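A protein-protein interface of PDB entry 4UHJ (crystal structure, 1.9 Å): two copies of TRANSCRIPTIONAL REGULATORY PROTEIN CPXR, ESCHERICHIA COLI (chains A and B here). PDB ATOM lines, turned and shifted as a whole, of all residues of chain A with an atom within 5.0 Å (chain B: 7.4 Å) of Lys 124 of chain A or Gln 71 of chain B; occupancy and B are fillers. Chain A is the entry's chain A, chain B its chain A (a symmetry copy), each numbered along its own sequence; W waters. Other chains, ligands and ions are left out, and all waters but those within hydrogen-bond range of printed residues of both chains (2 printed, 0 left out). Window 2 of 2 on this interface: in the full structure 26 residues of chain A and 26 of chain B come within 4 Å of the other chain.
The backbone carbonyl oxygen of Gln 71 of chain B sits at hydrogen-bond distance from the guanidinium group of Arg 117 of chain A (2.8 Å).
The guanidinium group (NE) of Arg 117 of chain A is in salt-bridge range of the side-chain carboxylate (OD1) of Asp 95 of chain B.
NZ of Lys 124 of chain A lies within hydrogen-bond range of OE1 of Gln 71 of chain B (2.8 Å).
Water W1 lies within hydrogen-bond range of the backbone carbonyl oxygen of Trp 120 of chain A (2.8 Å) and the side-chain amide nitrogen of Gln 71 of chain B (3.1 Å).
Water W2 lies within hydrogen-bond range of the backbone carbonyl oxygen of Gln 71 of chain B (3.3 Å) and the guanidinium group of Arg 117 of chain A (3.5 Å).
Of the 9 printed residues of chain A, 3 touch a printed residue of chain B.
Hydrophobic or aromatic side chains of chain A that line the printed part of chain B: Trp 120.
Printed residues of chain B that touch a printed residue of chain A: Arg 67, Gln 71, Thr 72, Pro 73 and Asp 95.
Among the printed residues, Asp or Glu carboxylates within 4 Å of a Lys or Arg side-chain nitrogen of the other chain: Arg 117 of chain A with Asp 95 of chain B (2.7 Å).
Arg 117 of chain A touches Arg 67 of chain B (NH2 to NH2, 3.6 Å).
Thr 72 of chain B touches Arg 117 of chain A.
Arg 117 of chain A touches Pro 73 of chain B.
CH2 of Trp 120 of chain A touches NE of Arg 67 of chain B (3.6 Å).
NE2 of Gln 71 of chain B touches CD1 of Trp 120 of chain A, at 3.3 Å.
Ala 127 of chain A touches none of the printed residues of chain B.
Printed residues of chain A within 4 Å of Arg 67 of chain B: Arg 117 and Trp 120.
Of chain A, only Arg 117 (2.8 Å), Trp 120 (3.3 Å) and Lys 124 (2.8 Å) come within 4 Å of Gln 71 of chain B.
Of the printed residues of chain A, Thr 72 of chain B touches Arg 117 (3.8 Å).
Printed residues of chain A within 4 Å of Pro 73 of chain B: Arg 117 (3.6 Å).
Of the printed residues of chain A, Asp 95 of chain B touches Arg 117 (2.7 Å).
The nearest printed residue of chain A that does not touch Arg 67 of chain B is Lys 124 of chain A (9.7 Å).
Position printed for both chains: 125.
Of the 8 pairs that touch across the chains among the printed residues, none has its exchanged pair printed and touching as well.
The backbone NH (N) of Leu 48 of chain B is in hydrogen-bond range of the backbone carbonyl oxygen (O) of Pro 73 of chain B.
OG of Ser 121 of chain A is in hydrogen-bond range of O of Arg 117 of chain A (3.2 Å).
The backbone carbonyl oxygen (O) of Val 74 of chain B is in hydrogen-bond range of the backbone NH (N) of Asp 95 of chain B (2.8 Å).
The guanidinium group (NE) of Arg 67 of chain B is in hydrogen-bond range of the backbone carbonyl oxygen (O) of Gly 93 of chain B, at 2.8 Å.
The backbone carbonyl oxygen (O) of Thr 72 of chain B lies within hydrogen-bond range of the guanidinium group (NH1) of Arg 67 of chain B (2.9 Å).
The backbone carbonyl oxygen (O) of His 70 of chain B is in hydrogen-bond range of the guanidinium group (NH1) of Arg 67 of chain B.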
ATOM      1  N   ARG A 117     -28.550 -26.507 -18.281  1.00  0.00           N
ATOM      2  CA  ARG A 117     -27.743 -27.720 -18.092  1.00  0.00           C
ATOM      3  C   ARG A 117     -27.505 -28.428 -19.439  1.00  0.00           C
ATOM      4  O   ARG A 117     -26.396 -28.898 -19.689  1.00  0.00           O
ATOM      5  CB  ARG A 117     -28.372 -28.710 -17.094  1.00  0.00           C
ATOM      6  CG  ARG A 117     -27.435 -29.934 -16.909  1.00  0.00           C
ATOM      7  CD  ARG A 117     -27.321 -30.560 -15.550  1.00  0.00           C
ATOM      8  NE  ARG A 117     -26.977 -29.599 -14.513  1.00  0.00           N
ATOM      9  CZ  ARG A 117     -25.755 -29.217 -14.180  1.00  0.00           C
ATOM     10  NH1 ARG A 117     -24.698 -29.674 -14.850  1.00  0.00           N
ATOM     11  NH2 ARG A 117     -25.578 -28.342 -13.212  1.00  0.00           N
ATOM     12  N   TRP A 120     -24.782 -26.539 -21.242  1.00  0.00           N
ATOM     13  CA  TRP A 120     -23.461 -26.820 -20.656  1.00  0.00           C
ATOM     14  C   TRP A 120     -22.907 -28.157 -21.187  1.00  0.00           C
ATOM     15  O   TRP A 120     -21.739 -28.220 -21.564  1.00  0.00           O
ATOM     16  CB  TRP A 120     -23.527 -26.836 -19.119  1.00  0.00           C
ATOM     17  CG  TRP A 120     -23.631 -25.484 -18.468  1.00  0.00           C
ATOM     18  CD1 TRP A 120     -23.185 -24.291 -18.966  1.00  0.00           C
ATOM     19  CD2 TRP A 120     -24.129 -25.206 -17.145  1.00  0.00           C
ATOM     20  NE1 TRP A 120     -23.397 -23.283 -18.044  1.00  0.00           N
ATOM     21  CE2 TRP A 120     -23.988 -23.818 -16.924  1.00  0.00           C
ATOM     22  CE3 TRP A 120     -24.672 -26.002 -16.120  1.00  0.00           C
ATOM     23  CZ2 TRP A 120     -24.369 -23.208 -15.716  1.00  0.00           C
ATOM     24  CZ3 TRP A 120     -25.068 -25.396 -14.932  1.00  0.00           C
ATOM     25  CH2 TRP A 120     -24.928 -24.014 -14.745  1.00  0.00           C
ATOM     26  N   SER A 121     -23.763 -29.202 -21.268  1.00  0.00           N
ATOM     27  CA  SER A 121     -23.406 -30.531 -21.789  1.00  0.00           C
ATOM     28  C   SER A 121     -23.014 -30.457 -23.272  1.00  0.00           C
ATOM     29  O   SER A 121     -22.005 -31.052 -23.659  1.00  0.00           O
ATOM     30  CB  SER A 121     -24.567 -31.509 -21.604  1.00  0.00           C
ATOM     31  OG  SER A 121     -24.838 -31.678 -20.227  1.00  0.00           O
ATOM     32  N   GLU A 122     -23.795 -29.695 -24.081  1.00  0.00           N
ATOM     33  CA  GLU A 122     -23.581 -29.486 -25.515  1.00  0.00           C
ATOM     34  C   GLU A 122     -22.261 -28.777 -25.788  1.00  0.00           C
ATOM     35  O   GLU A 122     -21.580 -29.150 -26.745  1.00  0.00           O
ATOM     36  CB  GLU A 122     -24.744 -28.694 -26.134  1.00  0.00           C
ATOM     37  CG  GLU A 122     -25.933 -29.570 -26.509  1.00  0.00           C
ATOM     38  CD  GLU A 122     -27.294 -28.900 -26.613  1.00  0.00           C
ATOM     39  OE1 GLU A 122     -27.361 -27.691 -26.940  1.00  0.00           O
ATOM     40  OE2 GLU A 122     -28.305 -29.604 -26.391  1.00  0.00           O
ATOM     41  N   GLN A 123     -21.904 -27.764 -24.961  1.00  0.00           N
ATOM     42  CA  GLN A 123     -20.654 -26.998 -25.066  1.00  0.00           C
ATOM     43  C   GLN A 123     -19.453 -27.912 -24.842  1.00  0.00           C
ATOM     44  O   GLN A 123     -18.480 -27.844 -25.601  1.00  0.00           O
ATOM     45  CB  GLN A 123     -20.613 -25.836 -24.057  1.00  0.00           C
ATOM     46  CG  GLN A 123     -21.587 -24.691 -24.324  1.00  0.00           C
ATOM     47  CD  GLN A 123     -21.273 -23.476 -23.472  1.00  0.00           C
ATOM     48  OE1 GLN A 123     -21.902 -23.197 -22.438  1.00  0.00           O
ATOM     49  NE2 GLN A 123     -20.269 -22.729 -23.890  1.00  0.00           N
ATOM     50  N   LYS A 124     -19.525 -28.764 -23.800  1.00  0.00           N
ATOM     51  CA  LYS A 124     -18.476 -29.721 -23.454  1.00  0.00           C
ATOM     52  C   LYS A 124     -18.319 -30.765 -24.561  1.00  0.00           C
ATOM     53  O   LYS A 124     -17.189 -31.050 -24.975  1.00  0.00           O
ATOM     54  CB  LYS A 124     -18.777 -30.397 -22.108  1.00  0.00           C
ATOM     55  CG  LYS A 124     -18.532 -29.489 -20.920  1.00  0.00           C
ATOM     56  CD  LYS A 124     -18.500 -30.260 -19.615  1.00  0.00           C
ATOM     57  CE  LYS A 124     -17.462 -29.717 -18.655  1.00  0.00           C
ATOM     58  NZ  LYS A 124     -17.783 -28.343 -18.175  1.00  0.00           N
ATOM     59  N   LEU A 125     -19.452 -31.287 -25.078  1.00  0.00           N
ATOM     60  CA  LEU A 125     -19.473 -32.301 -26.134  1.00  0.00           C
ATOM     61  C   LEU A 125     -18.824 -31.783 -27.429  1.00  0.00           C
ATOM     62  O   LEU A 125     -18.021 -32.503 -28.025  1.00  0.00           O
ATOM     63  CB  LEU A 125     -20.917 -32.782 -26.394  1.00  0.00           C
ATOM     64  CG  LEU A 125     -21.136 -33.887 -27.440  1.00  0.00           C
ATOM     65  CD1 LEU A 125     -20.376 -35.173 -27.085  1.00  0.00           C
ATOM     66  CD2 LEU A 125     -22.616 -34.187 -27.602  1.00  0.00           C
ATOM     67  N   ALA A 126     -19.147 -30.535 -27.837  1.00  0.00           N
ATOM     68  CA  ALA A 126     -18.602 -29.892 -29.039  1.00  0.00           C
ATOM     69  C   ALA A 126     -17.095 -29.618 -28.912  1.00  0.00           C
ATOM     70  O   ALA A 126     -16.383 -29.672 -29.917  1.00  0.00           O
ATOM     71  CB  ALA A 126     -19.342 -28.592 -29.317  1.00  0.00           C
ATOM     72  N   ALA A 127     -16.617 -29.331 -27.682  1.00  0.00           N
ATOM     73  CA  ALA A 127     -15.210 -29.061 -27.384  1.00  0.00           C
ATOM     74  C   ALA A 127     -14.361 -30.340 -27.456  1.00  0.00           C
ATOM     75  O   ALA A 127     -14.829 -31.437 -27.145  1.00  0.00           O
ATOM     76  CB  ALA A 127     -15.080 -28.426 -26.009  1.00  0.00           C
ATOM     77  N   LEU B  41     -15.778 -28.453  -2.182  1.00  0.00           N
ATOM     78  CA  LEU B  41     -16.244 -28.649  -3.560  1.00  0.00           C
ATOM     79  C   LEU B  41     -15.102 -28.803  -4.542  1.00  0.00           C
ATOM     80  O   LEU B  41     -14.276 -27.901  -4.709  1.00  0.00           O
ATOM     81  CB  LEU B  41     -17.188 -27.519  -4.016  1.00  0.00           C
ATOM     82  CG  LEU B  41     -17.815 -27.655  -5.428  1.00  0.00           C
ATOM     83  CD1 LEU B  41     -18.571 -28.970  -5.605  1.00  0.00           C
ATOM     84  CD2 LEU B  41     -18.757 -26.531  -5.701  1.00  0.00           C
ATOM     85  N   ASP B  43     -13.976 -31.640  -8.272  1.00  0.00           N
ATOM     86  CA  ASP B  43     -14.533 -32.435  -9.374  1.00  0.00           C
ATOM     87  C   ASP B  43     -15.077 -33.812  -8.938  1.00  0.00           C
ATOM     88  O   ASP B  43     -15.825 -34.401  -9.709  1.00  0.00           O
ATOM     89  CB  ASP B  43     -13.494 -32.605 -10.506  1.00  0.00           C
ATOM     90  CG  ASP B  43     -13.176 -31.343 -11.292  1.00  0.00           C
ATOM     91  OD1 ASP B  43     -13.806 -30.294 -11.026  1.00  0.00           O
ATOM     92  OD2 ASP B  43     -12.350 -31.417 -12.216  1.00  0.00           O
ATOM     93  N   ILE B  45     -17.291 -34.278  -6.587  1.00  0.00           N
ATOM     94  CA  ILE B  45     -18.689 -34.085  -6.162  1.00  0.00           C
ATOM     95  C   ILE B  45     -19.627 -34.207  -7.364  1.00  0.00           C
ATOM     96  O   ILE B  45     -19.445 -33.505  -8.363  1.00  0.00           O
ATOM     97  CB  ILE B  45     -18.878 -32.730  -5.428  1.00  0.00           C
ATOM     98  CG1 ILE B  45     -17.879 -32.563  -4.239  1.00  0.00           C
ATOM     99  CG2 ILE B  45     -20.355 -32.504  -4.988  1.00  0.00           C
ATOM    100  CD1 ILE B  45     -17.940 -33.665  -3.161  1.00  0.00           C
ATOM    101  N   ASP B  46     -20.631 -35.083  -7.254  1.00  0.00           N
ATOM    102  CA  ASP B  46     -21.607 -35.308  -8.329  1.00  0.00           C
ATOM    103  C   ASP B  46     -22.829 -34.465  -8.150  1.00  0.00           C
ATOM    104  O   ASP B  46     -23.523 -34.196  -9.127  1.00  0.00           O
ATOM    105  CB  ASP B  46     -22.000 -36.790  -8.423  1.00  0.00           C
ATOM    106  CG  ASP B  46     -20.781 -37.632  -8.753  1.00  0.00           C
ATOM    107  OD1 ASP B  46     -20.111 -37.329  -9.760  1.00  0.00           O
ATOM    108  OD2 ASP B  46     -20.460 -38.551  -7.966  1.00  0.00           O
ATOM    109  N   LEU B  48     -24.715 -31.364  -5.170  1.00  0.00           N
ATOM    110  CA  LEU B  48     -24.832 -30.616  -3.912  1.00  0.00           C
ATOM    111  C   LEU B  48     -26.282 -30.491  -3.505  1.00  0.00           C
ATOM    112  O   LEU B  48     -27.119 -30.153  -4.346  1.00  0.00           O
ATOM    113  CB  LEU B  48     -24.282 -29.188  -4.039  1.00  0.00           C
ATOM    114  CG  LEU B  48     -22.787 -28.989  -4.077  1.00  0.00           C
ATOM    115  CD1 LEU B  48     -22.348 -28.701  -5.493  1.00  0.00           C
ATOM    116  CD2 LEU B  48     -22.409 -27.805  -3.213  1.00  0.00           C
ATOM    117  N   LEU B  66     -19.834 -20.797  -6.282  1.00  0.00           N
ATOM    118  CA  LEU B  66     -19.500 -22.090  -6.877  1.00  0.00           C
ATOM    119  C   LEU B  66     -19.768 -22.116  -8.398  1.00  0.00           C
ATOM    120  O   LEU B  66     -19.017 -22.770  -9.119  1.00  0.00           O
ATOM    121  CB  LEU B  66     -20.201 -23.259  -6.158  1.00  0.00           C
ATOM    122  CG  LEU B  66     -21.673 -23.559  -6.433  1.00  0.00           C
ATOM    123  CD1 LEU B  66     -21.825 -24.518  -7.643  1.00  0.00           C
ATOM    124  CD2 LEU B  66     -22.319 -24.202  -5.193  1.00  0.00           C
ATOM    125  N   ARG B  67     -20.782 -21.375  -8.885  1.00  0.00           N
ATOM    126  CA  ARG B  67     -21.119 -21.336 -10.313  1.00  0.00           C
ATOM    127  C   ARG B  67     -20.057 -20.581 -11.145  1.00  0.00           C
ATOM    128  O   ARG B  67     -20.028 -20.725 -12.367  1.00  0.00           O
ATOM    129  CB  ARG B  67     -22.533 -20.758 -10.550  1.00  0.00           C
ATOM    130  CG  ARG B  67     -23.658 -21.762 -10.300  1.00  0.00           C
ATOM    131  CD  ARG B  67     -23.782 -22.762 -11.457  1.00  0.00           C
ATOM    132  NE  ARG B  67     -24.801 -23.783 -11.202  1.00  0.00           N
ATOM    133  CZ  ARG B  67     -24.553 -25.040 -10.837  1.00  0.00           C
ATOM    134  NH1 ARG B  67     -23.300 -25.464 -10.690  1.00  0.00           N
ATOM    135  NH2 ARG B  67     -25.548 -25.882 -10.627  1.00  0.00           N
ATOM    136  N   GLN B  68     -19.159 -19.846 -10.503  1.00  0.00           N
ATOM    137  CA  GLN B  68     -18.069 -19.181 -11.226  1.00  0.00           C
ATOM    138  C   GLN B  68     -17.018 -20.210 -11.695  1.00  0.00           C
ATOM    139  O   GLN B  68     -16.322 -19.950 -12.676  1.00  0.00           O
ATOM    140  CB  GLN B  68     -17.407 -18.112 -10.345  1.00  0.00           C
ATOM    141  CG  GLN B  68     -18.171 -16.794 -10.330  1.00  0.00           C
ATOM    142  CD  GLN B  68     -17.763 -15.908  -9.184  1.00  0.00           C
ATOM    143  OE1 GLN B  68     -16.582 -15.751  -8.858  1.00  0.00           O
ATOM    144  NE2 GLN B  68     -18.737 -15.278  -8.568  1.00  0.00           N
ATOM    145  N   THR B  69     -16.897 -21.371 -10.997  1.00  0.00           N
ATOM    146  CA  THR B  69     -15.884 -22.382 -11.347  1.00  0.00           C
ATOM    147  C   THR B  69     -16.425 -23.796 -11.586  1.00  0.00           C
ATOM    148  O   THR B  69     -15.732 -24.608 -12.214  1.00  0.00           O
ATOM    149  CB  THR B  69     -14.827 -22.471 -10.233  1.00  0.00           C
ATOM    150  OG1 THR B  69     -15.458 -22.832  -9.000  1.00  0.00           O
ATOM    151  CG2 THR B  69     -14.021 -21.189 -10.075  1.00  0.00           C
ATOM    152  N   HIS B  70     -17.636 -24.107 -11.084  1.00  0.00           N
ATOM    153  CA  HIS B  70     -18.185 -25.451 -11.182  1.00  0.00           C
ATOM    154  C   HIS B  70     -19.592 -25.464 -11.762  1.00  0.00           C
ATOM    155  O   HIS B  70     -20.428 -24.622 -11.410  1.00  0.00           O
ATOM    156  CB  HIS B  70     -18.200 -26.121  -9.783  1.00  0.00           C
ATOM    157  CG  HIS B  70     -16.829 -26.461  -9.254  1.00  0.00           C
ATOM    158  ND1 HIS B  70     -16.083 -25.538  -8.548  1.00  0.00           N
ATOM    159  CD2 HIS B  70     -16.126 -27.614  -9.340  1.00  0.00           C
ATOM    160  CE1 HIS B  70     -14.952 -26.152  -8.235  1.00  0.00           C
ATOM    161  NE2 HIS B  70     -14.933 -27.405  -8.689  1.00  0.00           N
ATOM    162  N   GLN B  71     -19.854 -26.461 -12.616  1.00  0.00           N
ATOM    163  CA  GLN B  71     -21.180 -26.703 -13.200  1.00  0.00           C
ATOM    164  C   GLN B  71     -21.858 -27.875 -12.470  1.00  0.00           C
ATOM    165  O   GLN B  71     -22.840 -28.424 -12.961  1.00  0.00           O
ATOM    166  CB  GLN B  71     -21.063 -26.989 -14.712  1.00  0.00           C
ATOM    167  CG  GLN B  71     -20.717 -25.763 -15.542  1.00  0.00           C
ATOM    168  CD  GLN B  71     -20.386 -26.122 -16.974  1.00  0.00           C
ATOM    169  OE1 GLN B  71     -20.247 -27.296 -17.352  1.00  0.00           O
ATOM    170  NE2 GLN B  71     -20.236 -25.114 -17.805  1.00  0.00           N
ATOM    171  N   THR B  72     -21.316 -28.274 -11.308  1.00  0.00           N
ATOM    172  CA  THR B  72     -21.856 -29.361 -10.474  1.00  0.00           C
ATOM    173  C   THR B  72     -23.380 -29.228 -10.275  1.00  0.00           C
ATOM    174  O   THR B  72     -23.840 -28.146  -9.887  1.00  0.00           O
ATOM    175  CB  THR B  72     -21.189 -29.365  -9.083  1.00  0.00           C
ATOM    176  OG1 THR B  72     -19.794 -29.106  -9.218  1.00  0.00           O
ATOM    177  CG2 THR B  72     -21.441 -30.665  -8.308  1.00  0.00           C
ATOM    178  N   PRO B  73     -24.161 -30.306 -10.484  1.00  0.00           N
ATOM    179  CA  PRO B  73     -25.610 -30.225 -10.200  1.00  0.00           C
ATOM    180  C   PRO B  73     -25.895 -29.757  -8.767  1.00  0.00           C
ATOM    181  O   PRO B  73     -25.187 -30.132  -7.827  1.00  0.00           O
ATOM    182  CB  PRO B  73     -26.085 -31.656 -10.417  1.00  0.00           C
ATOM    183  CG  PRO B  73     -25.123 -32.191 -11.472  1.00  0.00           C
ATOM    184  CD  PRO B  73     -23.797 -31.639 -11.016  1.00  0.00           C
ATOM    185  N   VAL B  74     -26.895 -28.874  -8.620  1.00  0.00           N
ATOM    186  CA  VAL B  74     -27.261 -28.308  -7.322  1.00  0.00           C
ATOM    187  C   VAL B  74     -28.777 -28.432  -7.127  1.00  0.00           C
ATOM    188  O   VAL B  74     -29.548 -28.003  -7.980  1.00  0.00           O
ATOM    189  CB  VAL B  74     -26.796 -26.817  -7.132  1.00  0.00           C
ATOM    190  CG1 VAL B  74     -27.383 -26.207  -5.844  1.00  0.00           C
ATOM    191  CG2 VAL B  74     -25.261 -26.681  -7.118  1.00  0.00           C
ATOM    192  N   GLY B  93     -28.660 -20.404 -10.617  1.00  0.00           N
ATOM    193  CA  GLY B  93     -27.838 -21.543 -11.006  1.00  0.00           C
ATOM    194  C   GLY B  93     -28.220 -22.909 -10.490  1.00  0.00           C
ATOM    195  O   GLY B  93     -27.565 -23.879 -10.844  1.00  0.00           O
ATOM    196  N   ASP B  95     -30.303 -26.398 -10.160  1.00  0.00           N
ATOM    197  CA  ASP B  95     -30.987 -27.280 -11.086  1.00  0.00           C
ATOM    198  C   ASP B  95     -32.379 -27.582 -10.616  1.00  0.00           C
ATOM    199  O   ASP B  95     -33.271 -27.787 -11.436  1.00  0.00           O
ATOM    200  CB  ASP B  95     -30.189 -28.569 -11.261  1.00  0.00           C
ATOM    201  CG  ASP B  95     -28.876 -28.299 -11.975  1.00  0.00           C
ATOM    202  OD1 ASP B  95     -28.896 -28.136 -13.227  1.00  0.00           O
ATOM    203  OD2 ASP B  95     -27.871 -28.099 -11.284  1.00  0.00           O
ATOM    204  N   SER B 118     -26.914 -36.638 -15.626  1.00  0.00           N
ATOM    205  CA  SER B 118     -25.452 -36.457 -15.589  1.00  0.00           C
ATOM    206  C   SER B 118     -24.756 -37.664 -16.187  1.00  0.00           C
ATOM    207  O   SER B 118     -23.811 -37.499 -16.964  1.00  0.00           O
ATOM    208  CB  SER B 118     -24.964 -36.241 -14.160  1.00  0.00           C
ATOM    209  OG  SER B 118     -25.360 -34.959 -13.715  1.00  0.00           O
ATOM    210  N   LEU B 125     -20.105 -38.044 -23.673  1.00  0.00           N
ATOM    211  CA  LEU B 125     -18.807 -37.368 -23.649  1.00  0.00           C
ATOM    212  C   LEU B 125     -17.647 -38.364 -23.815  1.00  0.00           C
ATOM    213  O   LEU B 125     -16.736 -38.097 -24.602  1.00  0.00           O
ATOM    214  CB  LEU B 125     -18.648 -36.546 -22.351  1.00  0.00           C
ATOM    215  CG  LEU B 125     -17.363 -35.723 -22.166  1.00  0.00           C
ATOM    216  CD1 LEU B 125     -17.178 -34.687 -23.284  1.00  0.00           C
ATOM    217  CD2 LEU B 125     -17.357 -35.033 -20.813  1.00  0.00           C
HETATM  218  O   HOH W   1     -20.137 -26.047 -20.710  1.00  0.00           O
HETATM  219  O   HOH W   2     -21.552 -31.099 -14.482  1.00  0.00           O
